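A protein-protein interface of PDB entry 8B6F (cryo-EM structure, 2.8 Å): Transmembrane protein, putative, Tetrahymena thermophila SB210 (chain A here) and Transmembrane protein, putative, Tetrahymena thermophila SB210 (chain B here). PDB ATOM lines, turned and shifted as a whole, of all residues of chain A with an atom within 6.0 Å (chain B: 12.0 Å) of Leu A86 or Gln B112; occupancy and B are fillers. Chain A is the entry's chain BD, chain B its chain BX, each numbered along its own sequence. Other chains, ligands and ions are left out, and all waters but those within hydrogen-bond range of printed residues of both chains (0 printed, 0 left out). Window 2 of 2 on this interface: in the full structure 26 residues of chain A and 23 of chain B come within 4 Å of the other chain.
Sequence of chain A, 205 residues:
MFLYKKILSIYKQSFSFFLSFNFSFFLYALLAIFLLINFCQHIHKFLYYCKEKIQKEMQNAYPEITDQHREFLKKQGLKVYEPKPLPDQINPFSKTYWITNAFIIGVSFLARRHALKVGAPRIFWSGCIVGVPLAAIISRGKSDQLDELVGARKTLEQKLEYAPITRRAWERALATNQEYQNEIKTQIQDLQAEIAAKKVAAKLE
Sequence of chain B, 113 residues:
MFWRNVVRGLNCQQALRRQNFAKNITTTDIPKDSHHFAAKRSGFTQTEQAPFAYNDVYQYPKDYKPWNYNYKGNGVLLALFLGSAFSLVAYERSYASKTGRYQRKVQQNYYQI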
ATOM      1  N   LYS A  84       1.702   4.147  -2.727  1.00  0.00           N
ATOM      2  CA  LYS A  84       1.441   4.628  -1.383  1.00  0.00           C
ATOM      3  C   LYS A  84       0.248   5.578  -1.368  1.00  0.00           C
ATOM      4  O   LYS A  84       0.029   6.328  -2.323  1.00  0.00           O
ATOM      5  CB  LYS A  84       2.672   5.347  -0.827  1.00  0.00           C
ATOM      6  CG  LYS A  84       3.856   4.418  -0.602  1.00  0.00           C
ATOM      7  CD  LYS A  84       5.085   5.167  -0.115  1.00  0.00           C
ATOM      8  CE  LYS A  84       5.722   5.980  -1.230  1.00  0.00           C
ATOM      9  NZ  LYS A  84       7.015   6.582  -0.800  1.00  0.00           N
ATOM     10  N   PRO A  85      -0.544   5.570  -0.297  1.00  0.00           N
ATOM     11  CA  PRO A  85      -1.701   6.468  -0.241  1.00  0.00           C
ATOM     12  C   PRO A  85      -1.275   7.924  -0.175  1.00  0.00           C
ATOM     13  O   PRO A  85      -0.194   8.262   0.313  1.00  0.00           O
ATOM     14  CB  PRO A  85      -2.420   6.038   1.042  1.00  0.00           C
ATOM     15  CG  PRO A  85      -1.354   5.441   1.886  1.00  0.00           C
ATOM     16  CD  PRO A  85      -0.402   4.777   0.936  1.00  0.00           C
ATOM     17  N   LEU A  86      -2.144   8.792  -0.681  1.00  0.00           N
ATOM     18  CA  LEU A  86      -1.860  10.217  -0.649  1.00  0.00           C
ATOM     19  C   LEU A  86      -1.729  10.687   0.799  1.00  0.00           C
ATOM     20  O   LEU A  86      -2.542  10.306   1.649  1.00  0.00           O
ATOM     21  CB  LEU A  86      -2.968  11.002  -1.353  1.00  0.00           C
ATOM     22  CG  LEU A  86      -3.129  10.786  -2.858  1.00  0.00           C
ATOM     23  CD1 LEU A  86      -4.368  11.497  -3.365  1.00  0.00           C
ATOM     24  CD2 LEU A  86      -1.900  11.267  -3.608  1.00  0.00           C
ATOM     25  N   PRO A  87      -0.728  11.504   1.119  1.00  0.00           N
ATOM     26  CA  PRO A  87      -0.633  12.047   2.476  1.00  0.00           C
ATOM     27  C   PRO A  87      -1.772  13.013   2.764  1.00  0.00           C
ATOM     28  O   PRO A  87      -2.427  13.539   1.861  1.00  0.00           O
ATOM     29  CB  PRO A  87       0.723  12.760   2.485  1.00  0.00           C
ATOM     30  CG  PRO A  87       1.002  13.061   1.069  1.00  0.00           C
ATOM     31  CD  PRO A  87       0.392  11.949   0.276  1.00  0.00           C
ATOM     32  N   ASP A  88      -2.001  13.241   4.058  1.00  0.00           N
ATOM     33  CA  ASP A  88      -3.136  14.058   4.470  1.00  0.00           C
ATOM     34  C   ASP A  88      -3.095  15.435   3.823  1.00  0.00           C
ATOM     35  O   ASP A  88      -4.139  15.992   3.465  1.00  0.00           O
ATOM     36  CB  ASP A  88      -3.162  14.181   5.993  1.00  0.00           C
ATOM     37  CG  ASP A  88      -3.381  12.849   6.679  1.00  0.00           C
ATOM     38  OD1 ASP A  88      -3.450  11.822   5.971  1.00  0.00           O
ATOM     39  OD2 ASP A  88      -3.489  12.826   7.922  1.00  0.00           O
ATOM     40  N   ILE A  90      -1.905  16.190   0.873  1.00  0.00           N
ATOM     41  CA  ILE A  90      -2.259  16.089  -0.538  1.00  0.00           C
ATOM     42  C   ILE A  90      -3.674  15.552  -0.719  1.00  0.00           C
ATOM     43  O   ILE A  90      -4.353  15.904  -1.689  1.00  0.00           O
ATOM     44  CB  ILE A  90      -1.235  15.208  -1.276  1.00  0.00           C
ATOM     45  CG1 ILE A  90       0.173  15.806  -1.176  1.00  0.00           C
ATOM     46  CG2 ILE A  90      -1.634  15.019  -2.736  1.00  0.00           C
ATOM     47  CD1 ILE A  90       0.329  17.172  -1.816  1.00  0.00           C
ATOM     48  N   ASN A  91      -4.141  14.705   0.190  1.00  0.00           N
ATOM     49  CA  ASN A  91      -5.458  14.100   0.056  1.00  0.00           C
ATOM     50  C   ASN A  91      -6.535  15.181   0.058  1.00  0.00           C
ATOM     51  O   ASN A  91      -6.592  15.979   1.004  1.00  0.00           O
ATOM     52  CB  ASN A  91      -5.689  13.116   1.201  1.00  0.00           C
ATOM     53  CG  ASN A  91      -6.948  12.296   1.026  1.00  0.00           C
ATOM     54  OD1 ASN A  91      -7.878  12.700   0.333  1.00  0.00           O
ATOM     55  ND2 ASN A  91      -6.987  11.135   1.665  1.00  0.00           N
ATOM     56  N   PRO A  92      -7.402  15.248  -0.959  1.00  0.00           N
ATOM     57  CA  PRO A  92      -8.437  16.292  -0.967  1.00  0.00           C
ATOM     58  C   PRO A  92      -9.650  15.983  -0.107  1.00  0.00           C
ATOM     59  O   PRO A  92     -10.527  16.847   0.022  1.00  0.00           O
ATOM     60  CB  PRO A  92      -8.824  16.381  -2.448  1.00  0.00           C
ATOM     61  CG  PRO A  92      -8.585  15.017  -2.967  1.00  0.00           C
ATOM     62  CD  PRO A  92      -7.403  14.471  -2.211  1.00  0.00           C
ATOM     63  N   SER A 143      -9.798  12.830  -8.644  1.00  0.00           N
ATOM     64  CA  SER A 143      -9.792  11.617  -7.834  1.00  0.00           C
ATOM     65  C   SER A 143     -10.956  10.702  -8.195  1.00  0.00           C
ATOM     66  O   SER A 143     -10.797   9.478  -8.252  1.00  0.00           O
ATOM     67  CB  SER A 143      -9.848  11.980  -6.349  1.00  0.00           C
ATOM     68  OG  SER A 143      -8.732  12.765  -5.969  1.00  0.00           O
ATOM     69  N   LEU A 149      -3.934   6.553 -14.566  1.00  0.00           N
ATOM     70  CA  LEU A 149      -2.576   6.979 -14.852  1.00  0.00           C
ATOM     71  C   LEU A 149      -1.609   5.981 -14.222  1.00  0.00           C
ATOM     72  O   LEU A 149      -2.009   4.974 -13.632  1.00  0.00           O
ATOM     73  CB  LEU A 149      -2.343   8.396 -14.330  1.00  0.00           C
ATOM     74  CG  LEU A 149      -1.145   9.165 -14.895  1.00  0.00           C
ATOM     75  CD1 LEU A 149      -1.604  10.475 -15.510  1.00  0.00           C
ATOM     76  CD2 LEU A 149      -0.101   9.422 -13.819  1.00  0.00           C
ATOM     77  N   VAL A 150      -0.316   6.251 -14.347  1.00  0.00           N
ATOM     78  CA  VAL A 150       0.680   5.392 -13.721  1.00  0.00           C
ATOM     79  C   VAL A 150       0.486   5.474 -12.215  1.00  0.00           C
ATOM     80  O   VAL A 150       0.718   6.520 -11.600  1.00  0.00           O
ATOM     81  CB  VAL A 150       2.105   5.786 -14.139  1.00  0.00           C
ATOM     82  CG1 VAL A 150       3.125   4.824 -13.555  1.00  0.00           C
ATOM     83  CG2 VAL A 150       2.192   5.810 -15.647  1.00  0.00           C
ATOM     84  N   GLY A 151       0.058   4.372 -11.616  1.00  0.00           N
ATOM     85  CA  GLY A 151      -0.264   4.359 -10.203  1.00  0.00           C
ATOM     86  C   GLY A 151      -1.162   3.178  -9.883  1.00  0.00           C
ATOM     87  O   GLY A 151      -1.241   2.217 -10.645  1.00  0.00           O
ATOM     88  N   ALA A 152      -1.835   3.280  -8.742  1.00  0.00           N
ATOM     89  CA  ALA A 152      -2.706   2.201  -8.296  1.00  0.00           C
ATOM     90  C   ALA A 152      -3.855   2.000  -9.275  1.00  0.00           C
ATOM     91  O   ALA A 152      -4.482   2.963  -9.725  1.00  0.00           O
ATOM     92  CB  ALA A 152      -3.246   2.510  -6.901  1.00  0.00           C
ATOM     93  N   LYS A 154      -7.585   0.958 -10.470  1.00  0.00           N
ATOM     94  CA  LYS A 154      -8.920   1.033  -9.898  1.00  0.00           C
ATOM     95  C   LYS A 154      -9.422  -0.371  -9.589  1.00  0.00           C
ATOM     96  O   LYS A 154      -9.357  -1.267 -10.435  1.00  0.00           O
ATOM     97  CB  LYS A 154      -9.870   1.740 -10.863  1.00  0.00           C
ATOM     98  CG  LYS A 154      -9.437   3.150 -11.242  1.00  0.00           C
ATOM     99  CD  LYS A 154      -9.445   4.084 -10.043  1.00  0.00           C
ATOM    100  CE  LYS A 154      -9.042   5.495 -10.439  1.00  0.00           C
ATOM    101  NZ  LYS A 154      -9.111   6.435  -9.286  1.00  0.00           N
ATOM    102  N   ARG B 104     -21.687  11.222  -0.471  1.00  0.00           N
ATOM    103  CA  ARG B 104     -20.423  10.597  -0.838  1.00  0.00           C
ATOM    104  C   ARG B 104     -19.982   9.613   0.238  1.00  0.00           C
ATOM    105  O   ARG B 104     -20.111   9.874   1.436  1.00  0.00           O
ATOM    106  CB  ARG B 104     -19.347  11.666  -1.040  1.00  0.00           C
ATOM    107  CG  ARG B 104     -17.942  11.111  -1.249  1.00  0.00           C
ATOM    108  CD  ARG B 104     -16.911  12.221  -1.303  1.00  0.00           C
ATOM    109  NE  ARG B 104     -17.066  13.056  -2.488  1.00  0.00           N
ATOM    110  CZ  ARG B 104     -16.519  12.797  -3.668  1.00  0.00           C
ATOM    111  NH1 ARG B 104     -15.776  11.721  -3.865  1.00  0.00           N
ATOM    112  NH2 ARG B 104     -16.721  13.640  -4.676  1.00  0.00           N
ATOM    113  N   GLN B 107     -13.624   6.995   0.984  1.00  0.00           N
ATOM    114  CA  GLN B 107     -12.841   5.799   1.242  1.00  0.00           C
ATOM    115  C   GLN B 107     -11.763   6.074   2.287  1.00  0.00           C
ATOM    116  O   GLN B 107     -11.437   7.221   2.602  1.00  0.00           O
ATOM    117  CB  GLN B 107     -12.205   5.292  -0.050  1.00  0.00           C
ATOM    118  CG  GLN B 107     -13.223   4.922  -1.117  1.00  0.00           C
ATOM    119  CD  GLN B 107     -12.589   4.305  -2.348  1.00  0.00           C
ATOM    120  OE1 GLN B 107     -13.128   3.359  -2.925  1.00  0.00           O
ATOM    121  NE2 GLN B 107     -11.446   4.841  -2.766  1.00  0.00           N
ATOM    122  N   GLN B 108     -11.209   4.988   2.831  1.00  0.00           N
ATOM    123  CA  GLN B 108     -10.188   5.102   3.866  1.00  0.00           C
ATOM    124  C   GLN B 108      -8.834   5.533   3.315  1.00  0.00           C
ATOM    125  O   GLN B 108      -8.030   6.099   4.063  1.00  0.00           O
ATOM    126  CB  GLN B 108     -10.040   3.772   4.608  1.00  0.00           C
ATOM    127  CG  GLN B 108     -11.240   3.398   5.470  1.00  0.00           C
ATOM    128  CD  GLN B 108     -12.456   2.993   4.658  1.00  0.00           C
ATOM    129  OE1 GLN B 108     -12.358   2.723   3.461  1.00  0.00           O
ATOM    130  NE2 GLN B 108     -13.614   2.951   5.307  1.00  0.00           N
ATOM    131  N   ASN B 109      -8.565   5.285   2.035  1.00  0.00           N
ATOM    132  CA  ASN B 109      -7.299   5.672   1.428  1.00  0.00           C
ATOM    133  C   ASN B 109      -7.536   6.072  -0.018  1.00  0.00           C
ATOM    134  O   ASN B 109      -8.322   5.436  -0.725  1.00  0.00           O
ATOM    135  CB  ASN B 109      -6.275   4.533   1.487  1.00  0.00           C
ATOM    136  CG  ASN B 109      -5.748   4.296   2.885  1.00  0.00           C
ATOM    137  OD1 ASN B 109      -5.505   5.238   3.638  1.00  0.00           O
ATOM    138  ND2 ASN B 109      -5.572   3.029   3.243  1.00  0.00           N
ATOM    139  N   TYR B 110      -6.856   7.131  -0.446  1.00  0.00           N
ATOM    140  CA  TYR B 110      -6.902   7.601  -1.822  1.00  0.00           C
ATOM    141  C   TYR B 110      -5.493   7.590  -2.393  1.00  0.00           C
ATOM    142  O   TYR B 110      -4.552   8.055  -1.742  1.00  0.00           O
ATOM    143  CB  TYR B 110      -7.497   9.007  -1.907  1.00  0.00           C
ATOM    144  CG  TYR B 110      -8.984   9.045  -1.657  1.00  0.00           C
ATOM    145  CD1 TYR B 110      -9.885   8.864  -2.696  1.00  0.00           C
ATOM    146  CD2 TYR B 110      -9.486   9.257  -0.382  1.00  0.00           C
ATOM    147  CE1 TYR B 110     -11.245   8.894  -2.472  1.00  0.00           C
ATOM    148  CE2 TYR B 110     -10.842   9.291  -0.147  1.00  0.00           C
ATOM    149  CZ  TYR B 110     -11.717   9.110  -1.197  1.00  0.00           C
ATOM    150  OH  TYR B 110     -13.071   9.143  -0.965  1.00  0.00           O
ATOM    151  N   TYR B 111      -5.352   7.059  -3.602  1.00  0.00           N
ATOM    152  CA  TYR B 111      -4.065   6.919  -4.264  1.00  0.00           C
ATOM    153  C   TYR B 111      -3.973   7.878  -5.442  1.00  0.00           C
ATOM    154  O   TYR B 111      -4.956   8.501  -5.853  1.00  0.00           O
ATOM    155  CB  TYR B 111      -3.856   5.475  -4.732  1.00  0.00           C
ATOM    156  CG  TYR B 111      -3.945   4.467  -3.614  1.00  0.00           C
ATOM    157  CD1 TYR B 111      -5.159   3.889  -3.268  1.00  0.00           C
ATOM    158  CD2 TYR B 111      -2.816   4.097  -2.900  1.00  0.00           C
ATOM    159  CE1 TYR B 111      -5.245   2.969  -2.243  1.00  0.00           C
ATOM    160  CE2 TYR B 111      -2.890   3.178  -1.873  1.00  0.00           C
ATOM    161  CZ  TYR B 111      -4.107   2.617  -1.550  1.00  0.00           C
ATOM    162  OH  TYR B 111      -4.181   1.702  -0.526  1.00  0.00           O
ATOM    163  N   GLN B 112      -2.765   7.997  -5.981  1.00  0.00           N
ATOM    164  CA  GLN B 112      -2.537   8.869  -7.121  1.00  0.00           C
ATOM    165  C   GLN B 112      -3.230   8.320  -8.363  1.00  0.00           C
ATOM    166  O   GLN B 112      -3.322   7.107  -8.566  1.00  0.00           O
ATOM    167  CB  GLN B 112      -1.041   9.025  -7.381  1.00  0.00           C
ATOM    168  CG  GLN B 112      -0.307   9.780  -6.287  1.00  0.00           C
ATOM    169  CD  GLN B 112       1.178   9.872  -6.543  1.00  0.00           C
ATOM    170  OE1 GLN B 112       1.740   9.073  -7.291  1.00  0.00           O
ATOM    171  NE2 GLN B 112       1.826  10.851  -5.925  1.00  0.00           N
ATOM    172  N   ILE B 113      -3.722   9.229  -9.195  1.00  0.00           N
ATOM    173  CA  ILE B 113      -4.414   8.854 -10.420  1.00  0.00           C
ATOM    174  C   ILE B 113      -4.747  10.097 -11.233  1.00  0.00           C
ATOM    175  O   ILE B 113      -5.773  10.738 -11.009  1.00  0.00           O
ATOM    176  CB  ILE B 113      -5.688   8.050 -10.113  1.00  0.00           C
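The backbone NH of Leu A86 sits at hydrogen-bond distance from the backbone carbonyl oxygen of Tyr B110 (2.7 Å).
N of Gln B107 lies within hydrogen-bond range of OH of Tyr B110 (3.0 Å).
Among the printed residues, pairs that only touch across the chains: Lys A84 with Tyr B111 (3.7 Å), Pro A85 with Tyr B110 (3.6 Å), Pro A85 with Tyr B111 (3.7 Å), Leu A86 with Tyr B111 (3.9 Å), Leu A86 with Gln B112 (3.5 Å), Asn A91 with Tyr B110 (3.7 Å), Ala A152 with Tyr B111 (3.7 Å) and Lys A154 with Ile B113 (3.9 Å).
Of the printed residues of chain B, Lys A84 touches Tyr B111 (3.7 Å). No residue of chain B comes within 4 Å of Asp A88. Ile A90 touches none of the printed residues of chain B. Of chain B, only Tyr B110 comes within 4 Å of Asn A91. No residue of chain B comes within 4 Å of Leu A149. Of chain B, only Tyr B111 comes within 4 Å of Ala A152. Of the printed residues of chain B, Lys A154 touches Ile B113 (3.9 Å). Asn B109 touches none of the printed residues of chain A. Gln B112 touches just one residue of chain A: Leu A86 (3.5 Å). Of the printed residues of chain A, Ile B113 touches Lys A154 (3.9 Å). The nearest residue of chain B that does not touch Leu A86 is Asn B109 (6.1 Å). The nearest residue of chain A that does not touch Gln B112 is Ala A152 (4.1 Å). The nearest printed residue of chain A that does not touch Ile B113 is Leu A149 (4.3 Å).
Of the 14 printed residues of chain A, 6 touch a printed residue of chain B. Of the 8 printed residues of chain B, 4 touch a printed residue of chain A. Printed residues of chain B that touch a printed residue of chain A: Tyr B110, Tyr B111, Gln B112 and Ile B113. Hydrophobic or aromatic side chains of chain B that line the printed part of chain A: Tyr B110, Tyr B111 and Ile B113. Along chain B the printed residues that touch a printed residue of chain A span positions 110 to 113. Among the printed residues, no Asp or Glu carboxylate lies within 4 Å of a Lys or Arg side-chain nitrogen of the other chain.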
